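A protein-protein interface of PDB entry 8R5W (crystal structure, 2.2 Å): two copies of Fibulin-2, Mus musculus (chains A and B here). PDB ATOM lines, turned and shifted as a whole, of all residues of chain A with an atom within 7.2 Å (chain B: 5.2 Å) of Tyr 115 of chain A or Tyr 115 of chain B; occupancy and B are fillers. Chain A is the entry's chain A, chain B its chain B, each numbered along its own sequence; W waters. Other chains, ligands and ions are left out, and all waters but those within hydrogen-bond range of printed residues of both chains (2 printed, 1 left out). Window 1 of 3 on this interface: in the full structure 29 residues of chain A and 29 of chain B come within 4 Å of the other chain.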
ATOM      1  N   GLN A  50     -20.768  -9.894 -20.139  1.00  0.00           N
ATOM      2  CA  GLN A  50     -21.282 -11.199 -20.494  1.00  0.00           C
ATOM      3  C   GLN A  50     -22.805 -11.151 -20.612  1.00  0.00           C
ATOM      4  O   GLN A  50     -23.356 -11.768 -21.529  1.00  0.00           O
ATOM      5  CB  GLN A  50     -20.857 -12.284 -19.504  1.00  0.00           C
ATOM      6  CG  GLN A  50     -19.391 -12.686 -19.616  1.00  0.00           C
ATOM      7  CD  GLN A  50     -19.035 -13.183 -20.993  1.00  0.00           C
ATOM      8  OE1 GLN A  50     -18.113 -12.697 -21.663  1.00  0.00           O
ATOM      9  NE2 GLN A  50     -19.772 -14.192 -21.426  1.00  0.00           N
ATOM     10  N   SER A  54     -24.828 -11.746 -24.068  1.00  0.00           N
ATOM     11  CA  SER A  54     -25.789 -12.854 -24.141  1.00  0.00           C
ATOM     12  C   SER A  54     -27.148 -12.368 -24.626  1.00  0.00           C
ATOM     13  O   SER A  54     -27.811 -13.080 -25.361  1.00  0.00           O
ATOM     14  CB  SER A  54     -25.978 -13.562 -22.834  1.00  0.00           C
ATOM     15  OG  SER A  54     -24.711 -14.051 -22.417  1.00  0.00           O
ATOM     16  N   LYS A  57     -26.946 -11.664 -28.257  1.00  0.00           N
ATOM     17  CA  LYS A  57     -26.760 -12.915 -28.964  1.00  0.00           C
ATOM     18  C   LYS A  57     -28.084 -13.660 -29.084  1.00  0.00           C
ATOM     19  O   LYS A  57     -28.421 -14.150 -30.170  1.00  0.00           O
ATOM     20  CB  LYS A  57     -25.726 -13.862 -28.351  1.00  0.00           C
ATOM     21  CG  LYS A  57     -24.277 -13.500 -28.597  1.00  0.00           C
ATOM     22  CD  LYS A  57     -23.284 -14.502 -28.007  1.00  0.00           C
ATOM     23  CE  LYS A  57     -21.888 -14.173 -28.431  1.00  0.00           C
ATOM     24  NZ  LYS A  57     -20.964 -15.151 -27.839  1.00  0.00           N
ATOM     25  N   GLU A  58     -28.837 -13.762 -27.989  1.00  0.00           N
ATOM     26  CA  GLU A  58     -30.069 -14.541 -28.009  1.00  0.00           C
ATOM     27  C   GLU A  58     -31.085 -13.846 -28.925  1.00  0.00           C
ATOM     28  O   GLU A  58     -31.775 -14.507 -29.688  1.00  0.00           O
ATOM     29  CB  GLU A  58     -30.590 -14.811 -26.600  1.00  0.00           C
ATOM     30  CG  GLU A  58     -31.682 -15.877 -26.527  1.00  0.00           C
ATOM     31  CD  GLU A  58     -33.094 -15.365 -26.735  1.00  0.00           C
ATOM     32  OE1 GLU A  58     -33.272 -14.165 -27.027  1.00  0.00           O
ATOM     33  OE2 GLU A  58     -34.027 -16.178 -26.575  1.00  0.00           O
ATOM     34  N   LEU A  86     -25.630 -13.367 -33.833  1.00  0.00           N
ATOM     35  CA  LEU A  86     -25.792 -14.736 -34.299  1.00  0.00           C
ATOM     36  C   LEU A  86     -26.855 -14.832 -35.387  1.00  0.00           C
ATOM     37  O   LEU A  86     -27.470 -15.887 -35.569  1.00  0.00           O
ATOM     38  CB  LEU A  86     -26.193 -15.654 -33.152  1.00  0.00           C
ATOM     39  CG  LEU A  86     -25.211 -15.667 -31.979  1.00  0.00           C
ATOM     40  CD1 LEU A  86     -25.582 -16.739 -30.982  1.00  0.00           C
ATOM     41  CD2 LEU A  86     -23.795 -15.859 -32.460  1.00  0.00           C
ATOM     42  N   GLN A  89     -25.514 -17.230 -38.174  1.00  0.00           N
ATOM     43  CA  GLN A  89     -25.309 -18.556 -37.636  1.00  0.00           C
ATOM     44  C   GLN A  89     -26.654 -19.239 -37.426  1.00  0.00           C
ATOM     45  O   GLN A  89     -26.839 -20.363 -37.861  1.00  0.00           O
ATOM     46  CB  GLN A  89     -24.546 -18.451 -36.321  1.00  0.00           C
ATOM     47  CG  GLN A  89     -24.352 -19.778 -35.594  1.00  0.00           C
ATOM     48  CD  GLN A  89     -23.496 -19.601 -34.357  1.00  0.00           C
ATOM     49  OE1 GLN A  89     -23.890 -18.933 -33.397  1.00  0.00           O
ATOM     50  NE2 GLN A  89     -22.270 -20.085 -34.439  1.00  0.00           N
ATOM     51  N   CYS A  90     -27.590 -18.564 -36.751  1.00  0.00           N
ATOM     52  CA  CYS A  90     -28.845 -19.187 -36.400  1.00  0.00           C
ATOM     53  C   CYS A  90     -29.725 -19.366 -37.638  1.00  0.00           C
ATOM     54  O   CYS A  90     -30.425 -20.359 -37.755  1.00  0.00           O
ATOM     55  CB  CYS A  90     -29.498 -18.434 -35.256  1.00  0.00           C
ATOM     56  SG  CYS A  90     -28.609 -18.692 -33.705  1.00  0.00           S
ATOM     57  N   PRO A 111     -24.266 -32.822 -31.660  1.00  0.00           N
ATOM     58  CA  PRO A 111     -23.521 -31.931 -30.773  1.00  0.00           C
ATOM     59  C   PRO A 111     -22.282 -31.288 -31.390  1.00  0.00           C
ATOM     60  O   PRO A 111     -21.823 -30.256 -30.919  1.00  0.00           O
ATOM     61  CB  PRO A 111     -23.103 -32.857 -29.587  1.00  0.00           C
ATOM     62  CG  PRO A 111     -24.023 -34.039 -29.648  1.00  0.00           C
ATOM     63  CD  PRO A 111     -24.450 -34.165 -31.089  1.00  0.00           C
ATOM     64  N   ASN A 112     -21.721 -31.894 -32.438  1.00  0.00           N
ATOM     65  CA  ASN A 112     -20.542 -31.328 -33.067  1.00  0.00           C
ATOM     66  C   ASN A 112     -20.846 -29.965 -33.687  1.00  0.00           C
ATOM     67  O   ASN A 112     -19.935 -29.171 -33.882  1.00  0.00           O
ATOM     68  CB  ASN A 112     -19.972 -32.290 -34.095  1.00  0.00           C
ATOM     69  CG  ASN A 112     -19.495 -33.566 -33.437  1.00  0.00           C
ATOM     70  OD1 ASN A 112     -18.600 -33.541 -32.589  1.00  0.00           O
ATOM     71  ND2 ASN A 112     -20.091 -34.682 -33.810  1.00  0.00           N
ATOM     72  N   LEU A 113     -22.121 -29.705 -34.020  1.00  0.00           N
ATOM     73  CA  LEU A 113     -22.539 -28.415 -34.553  1.00  0.00           C
ATOM     74  C   LEU A 113     -22.375 -27.312 -33.508  1.00  0.00           C
ATOM     75  O   LEU A 113     -22.349 -26.147 -33.881  1.00  0.00           O
ATOM     76  CB  LEU A 113     -23.991 -28.476 -35.030  1.00  0.00           C
ATOM     77  CG  LEU A 113     -24.261 -29.258 -36.305  1.00  0.00           C
ATOM     78  CD1 LEU A 113     -25.750 -29.467 -36.492  1.00  0.00           C
ATOM     79  CD2 LEU A 113     -23.648 -28.552 -37.520  1.00  0.00           C
ATOM     80  N   GLY A 114     -22.313 -27.681 -32.222  1.00  0.00           N
ATOM     81  CA  GLY A 114     -22.084 -26.722 -31.149  1.00  0.00           C
ATOM     82  C   GLY A 114     -23.362 -26.016 -30.701  1.00  0.00           C
ATOM     83  O   GLY A 114     -24.452 -26.415 -31.104  1.00  0.00           O
ATOM     84  N   TYR A 115     -23.202 -24.990 -29.859  1.00  0.00           N
ATOM     85  CA  TYR A 115     -24.297 -24.210 -29.307  1.00  0.00           C
ATOM     86  C   TYR A 115     -24.227 -22.786 -29.869  1.00  0.00           C
ATOM     87  O   TYR A 115     -23.152 -22.181 -29.869  1.00  0.00           O
ATOM     88  CB  TYR A 115     -24.176 -24.134 -27.782  1.00  0.00           C
ATOM     89  CG  TYR A 115     -25.294 -23.339 -27.109  1.00  0.00           C
ATOM     90  CD1 TYR A 115     -26.514 -23.921 -26.781  1.00  0.00           C
ATOM     91  CD2 TYR A 115     -25.144 -21.974 -26.877  1.00  0.00           C
ATOM     92  CE1 TYR A 115     -27.541 -23.176 -26.229  1.00  0.00           C
ATOM     93  CE2 TYR A 115     -26.160 -21.222 -26.311  1.00  0.00           C
ATOM     94  CZ  TYR A 115     -27.346 -21.834 -25.950  1.00  0.00           C
ATOM     95  OH  TYR A 115     -28.338 -21.077 -25.397  1.00  0.00           O
ATOM     96  N   PRO A 116     -25.347 -22.194 -30.334  1.00  0.00           N
ATOM     97  CA  PRO A 116     -26.667 -22.829 -30.295  1.00  0.00           C
ATOM     98  C   PRO A 116     -27.118 -23.587 -31.543  1.00  0.00           C
ATOM     99  O   PRO A 116     -28.281 -23.958 -31.675  1.00  0.00           O
ATOM    100  CB  PRO A 116     -27.536 -21.576 -30.073  1.00  0.00           C
ATOM    101  CG  PRO A 116     -26.901 -20.506 -30.944  1.00  0.00           C
ATOM    102  CD  PRO A 116     -25.406 -20.835 -30.893  1.00  0.00           C
ATOM    103  N   CYS A 117     -26.171 -23.866 -32.443  1.00  0.00           N
ATOM    104  CA  CYS A 117     -26.475 -24.380 -33.768  1.00  0.00           C
ATOM    105  C   CYS A 117     -27.272 -25.677 -33.672  1.00  0.00           C
ATOM    106  O   CYS A 117     -28.287 -25.814 -34.326  1.00  0.00           O
ATOM    107  CB  CYS A 117     -25.204 -24.593 -34.574  1.00  0.00           C
ATOM    108  SG  CYS A 117     -25.516 -25.081 -36.287  1.00  0.00           S
ATOM    109  N   ASN A 118     -26.824 -26.620 -32.841  1.00  0.00           N
ATOM    110  CA  ASN A 118     -27.466 -27.917 -32.728  1.00  0.00           C
ATOM    111  C   ASN A 118     -28.910 -27.748 -32.276  1.00  0.00           C
ATOM    112  O   ASN A 118     -29.838 -28.272 -32.921  1.00  0.00           O
ATOM    113  CB  ASN A 118     -26.728 -28.832 -31.760  1.00  0.00           C
ATOM    114  CG  ASN A 118     -27.256 -30.252 -31.783  1.00  0.00           C
ATOM    115  OD1 ASN A 118     -27.794 -30.713 -32.791  1.00  0.00           O
ATOM    116  ND2 ASN A 118     -27.064 -30.990 -30.706  1.00  0.00           N
ATOM    117  N   HIS A 119     -29.089 -27.026 -31.166  1.00  0.00           N
ATOM    118  CA  HIS A 119     -30.411 -26.768 -30.625  1.00  0.00           C
ATOM    119  C   HIS A 119     -31.293 -26.102 -31.683  1.00  0.00           C
ATOM    120  O   HIS A 119     -32.465 -26.424 -31.819  1.00  0.00           O
ATOM    121  CB  HIS A 119     -30.332 -25.903 -29.365  1.00  0.00           C
ATOM    122  CG  HIS A 119     -31.676 -25.725 -28.733  1.00  0.00           C
ATOM    123  ND1 HIS A 119     -32.469 -24.606 -28.898  1.00  0.00           N
ATOM    124  CD2 HIS A 119     -32.393 -26.576 -27.984  1.00  0.00           C
ATOM    125  CE1 HIS A 119     -33.609 -24.780 -28.254  1.00  0.00           C
ATOM    126  NE2 HIS A 119     -33.578 -25.960 -27.671  1.00  0.00           N
ATOM    127  N   VAL A 120     -30.736 -25.142 -32.427  1.00  0.00           N
ATOM    128  CA  VAL A 120     -31.539 -24.409 -33.390  1.00  0.00           C
ATOM    129  C   VAL A 120     -31.898 -25.322 -34.559  1.00  0.00           C
ATOM    130  O   VAL A 120     -33.006 -25.294 -35.052  1.00  0.00           O
ATOM    131  CB  VAL A 120     -30.813 -23.143 -33.858  1.00  0.00           C
ATOM    132  CG1 VAL A 120     -31.392 -22.596 -35.155  1.00  0.00           C
ATOM    133  CG2 VAL A 120     -30.817 -22.084 -32.781  1.00  0.00           C
ATOM    134  N   SER B  54     -17.153 -24.860 -33.550  1.00  0.00           N
ATOM    135  CA  SER B  54     -17.503 -25.493 -32.287  1.00  0.00           C
ATOM    136  C   SER B  54     -16.296 -26.176 -31.663  1.00  0.00           C
ATOM    137  O   SER B  54     -16.137 -26.125 -30.457  1.00  0.00           O
ATOM    138  CB  SER B  54     -18.611 -26.485 -32.426  1.00  0.00           C
ATOM    139  OG  SER B  54     -19.746 -25.831 -32.970  1.00  0.00           O
ATOM    140  N   GLN B  89     -12.994 -15.699 -22.238  1.00  0.00           N
ATOM    141  CA  GLN B  89     -14.349 -15.772 -21.720  1.00  0.00           C
ATOM    142  C   GLN B  89     -14.467 -16.868 -20.660  1.00  0.00           C
ATOM    143  O   GLN B  89     -14.959 -16.609 -19.574  1.00  0.00           O
ATOM    144  CB  GLN B  89     -15.315 -16.029 -22.874  1.00  0.00           C
ATOM    145  CG  GLN B  89     -16.769 -16.175 -22.439  1.00  0.00           C
ATOM    146  CD  GLN B  89     -17.732 -16.062 -23.602  1.00  0.00           C
ATOM    147  OE1 GLN B  89     -18.371 -17.043 -23.964  1.00  0.00           O
ATOM    148  NE2 GLN B  89     -17.801 -14.894 -24.235  1.00  0.00           N
ATOM    149  N   LEU B 113     -25.893 -14.771 -17.894  1.00  0.00           N
ATOM    150  CA  LEU B 113     -24.480 -14.805 -18.256  1.00  0.00           C
ATOM    151  C   LEU B 113     -24.268 -15.478 -19.608  1.00  0.00           C
ATOM    152  O   LEU B 113     -23.206 -15.339 -20.201  1.00  0.00           O
ATOM    153  CB  LEU B 113     -23.644 -15.508 -17.178  1.00  0.00           C
ATOM    154  CG  LEU B 113     -23.450 -14.730 -15.880  1.00  0.00           C
ATOM    155  CD1 LEU B 113     -22.917 -15.655 -14.766  1.00  0.00           C
ATOM    156  CD2 LEU B 113     -22.516 -13.562 -16.129  1.00  0.00           C
ATOM    157  N   GLY B 114     -25.248 -16.286 -20.037  1.00  0.00           N
ATOM    158  CA  GLY B 114     -25.200 -16.946 -21.326  1.00  0.00           C
ATOM    159  C   GLY B 114     -24.456 -18.278 -21.225  1.00  0.00           C
ATOM    160  O   GLY B 114     -24.068 -18.711 -20.138  1.00  0.00           O
ATOM    161  N   TYR B 115     -24.283 -18.910 -22.389  1.00  0.00           N
ATOM    162  CA  TYR B 115     -23.585 -20.180 -22.524  1.00  0.00           C
ATOM    163  C   TYR B 115     -22.313 -19.944 -23.323  1.00  0.00           C
ATOM    164  O   TYR B 115     -22.367 -19.315 -24.383  1.00  0.00           O
ATOM    165  CB  TYR B 115     -24.458 -21.200 -23.268  1.00  0.00           C
ATOM    166  CG  TYR B 115     -23.807 -22.564 -23.395  1.00  0.00           C
ATOM    167  CD1 TYR B 115     -23.948 -23.510 -22.389  1.00  0.00           C
ATOM    168  CD2 TYR B 115     -23.045 -22.901 -24.510  1.00  0.00           C
ATOM    169  CE1 TYR B 115     -23.354 -24.758 -22.477  1.00  0.00           C
ATOM    170  CE2 TYR B 115     -22.422 -24.138 -24.605  1.00  0.00           C
ATOM    171  CZ  TYR B 115     -22.584 -25.067 -23.587  1.00  0.00           C
ATOM    172  OH  TYR B 115     -21.970 -26.286 -23.682  1.00  0.00           O
ATOM    173  N   PRO B 116     -21.140 -20.454 -22.896  1.00  0.00           N
ATOM    174  CA  PRO B 116     -21.022 -21.314 -21.721  1.00  0.00           C
ATOM    175  C   PRO B 116     -20.677 -20.651 -20.397  1.00  0.00           C
ATOM    176  O   PRO B 116     -20.408 -21.375 -19.444  1.00  0.00           O
ATOM    177  CB  PRO B 116     -19.867 -22.213 -22.215  1.00  0.00           C
ATOM    178  CG  PRO B 116     -18.930 -21.273 -22.932  1.00  0.00           C
ATOM    179  CD  PRO B 116     -19.837 -20.196 -23.541  1.00  0.00           C
ATOM    180  N   CYS B 117     -20.774 -19.317 -20.312  1.00  0.00           N
ATOM    181  CA  CYS B 117     -20.289 -18.596 -19.133  1.00  0.00           C
ATOM    182  C   CYS B 117     -20.953 -19.133 -17.855  1.00  0.00           C
ATOM    183  O   CYS B 117     -20.272 -19.448 -16.891  1.00  0.00           O
ATOM    184  CB  CYS B 117     -20.520 -17.098 -19.271  1.00  0.00           C
ATOM    185  SG  CYS B 117     -19.803 -16.132 -17.915  1.00  0.00           S
ATOM    186  N   ASN B 118     -22.273 -19.249 -17.865  1.00  0.00           N
ATOM    187  CA  ASN B 118     -23.014 -19.668 -16.682  1.00  0.00           C
ATOM    188  C   ASN B 118     -22.561 -21.065 -16.236  1.00  0.00           C
ATOM    189  O   ASN B 118     -22.196 -21.268 -15.075  1.00  0.00           O
ATOM    190  CB  ASN B 118     -24.520 -19.699 -16.934  1.00  0.00           C
ATOM    191  CG  ASN B 118     -25.294 -19.893 -15.649  1.00  0.00           C
ATOM    192  OD1 ASN B 118     -24.842 -19.508 -14.559  1.00  0.00           O
ATOM    193  ND2 ASN B 118     -26.486 -20.456 -15.746  1.00  0.00           N
ATOM    194  N   HIS B 119     -22.594 -22.007 -17.183  1.00  0.00           N
ATOM    195  CA  HIS B 119     -22.188 -23.374 -16.927  1.00  0.00           C
ATOM    196  C   HIS B 119     -20.759 -23.409 -16.382  1.00  0.00           C
ATOM    197  O   HIS B 119     -20.443 -24.160 -15.469  1.00  0.00           O
ATOM    198  CB  HIS B 119     -22.280 -24.236 -18.189  1.00  0.00           C
ATOM    199  CG  HIS B 119     -22.103 -25.675 -17.821  1.00  0.00           C
ATOM    200  ND1 HIS B 119     -22.839 -26.197 -16.775  1.00  0.00           N
ATOM    201  CD2 HIS B 119     -21.320 -26.683 -18.266  1.00  0.00           C
ATOM    202  CE1 HIS B 119     -22.522 -27.481 -16.614  1.00  0.00           C
ATOM    203  NE2 HIS B 119     -21.605 -27.788 -17.510  1.00  0.00           N
HETATM  204  O   HOH W   1     -19.521 -17.625 -26.128  1.00  0.00           O
HETATM  205  O   HOH W   2     -21.627 -16.836 -22.281  1.00  0.00           O
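The side-chain amide oxygen (OE1) of Gln 50 of chain A lies within hydrogen-bond range of the side-chain amide nitrogen (NE2) of Gln 89 of chain B, at 3.4 Å.
OG of Ser 54 of chain A sits at hydrogen-bond distance from O of Leu 113 of chain B.
OG of Ser 54 of chain A lies close to N of Gly 114 of chain B (3.3 Å).
O of Asn 112 of chain A lies close to OG of Ser 54 of chain B.
The backbone carbonyl oxygen of Leu 113 of chain A sits at hydrogen-bond distance from the side-chain hydroxyl of Ser 54 of chain B (2.8 Å).
N of Gly 114 of chain A lies close to OG of Ser 54 of chain B, at 3.3 Å.
The side-chain hydroxyl (OG) of Ser 54 of chain A is in hydrogen-bond range of the backbone carbonyl oxygen (O) of Gln 50 of chain A (2.8 Å).
Leu 113 of chain B touches Gln 50 of chain A.
NE2 of Gln 50 of chain A touches CB of Cys 117 of chain B, at 3.7 Å.
Tyr 115 of chain B touches Tyr 115 of chain A (CD2 to CD2, 3.3 Å).
Of the printed residues of chain B, Leu 113 of chain A touches Ser 54 (2.8 Å).
Of the printed residues of chain B, Gly 114 of chain A touches Ser 54 (3.1 Å).
Tyr 115 of chain A touches one residue of chain B.
Of the printed residues of chain A, Gln 89 of chain B touches Gln 50.
Of chain A, only Tyr 115 comes within 4 Å of Tyr 115 of chain B.
The nearest residue of chain A that does not touch Tyr 115 of chain B is Ser 54 of chain A (4.9 Å).
Hydrophobic or aromatic side chains of chain B that line the printed part of chain A: Leu 113 and Tyr 115.
Among the printed residues, 9 pairs touch across the chains.
Among the printed residues, no Asp or Glu carboxylate lies within 4 Å of a Lys or Arg side-chain nitrogen of the other chain.
Ser 54 of chain A touches Leu 113 of chain B, and with the chains exchanged Leu 113 of chain A touches Ser 54 of chain B.
Ser 54 of chain A touches Gly 114 of chain B, and with the chains exchanged Gly 114 of chain A touches Ser 54 of chain B.
Tyr 115 of chain B touches its own counterpart, Tyr 115 of chain A.
Of the 9 pairs that touch across the chains among the printed residues, 5 have their exchanged pair printed and touching as well.
Water W1 lies within hydrogen-bond range of OE1 of Gln 89 of chain B and NZ of Lys 57 of chain A.
Water W2 lies within hydrogen-bond range of O of Leu 113 of chain B (3.0 Å), N of Cys 117 of chain B (3.3 Å), O of Tyr 115 of chain B (3.3 Å) and NE2 of Gln 50 of chain A (3.3 Å).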
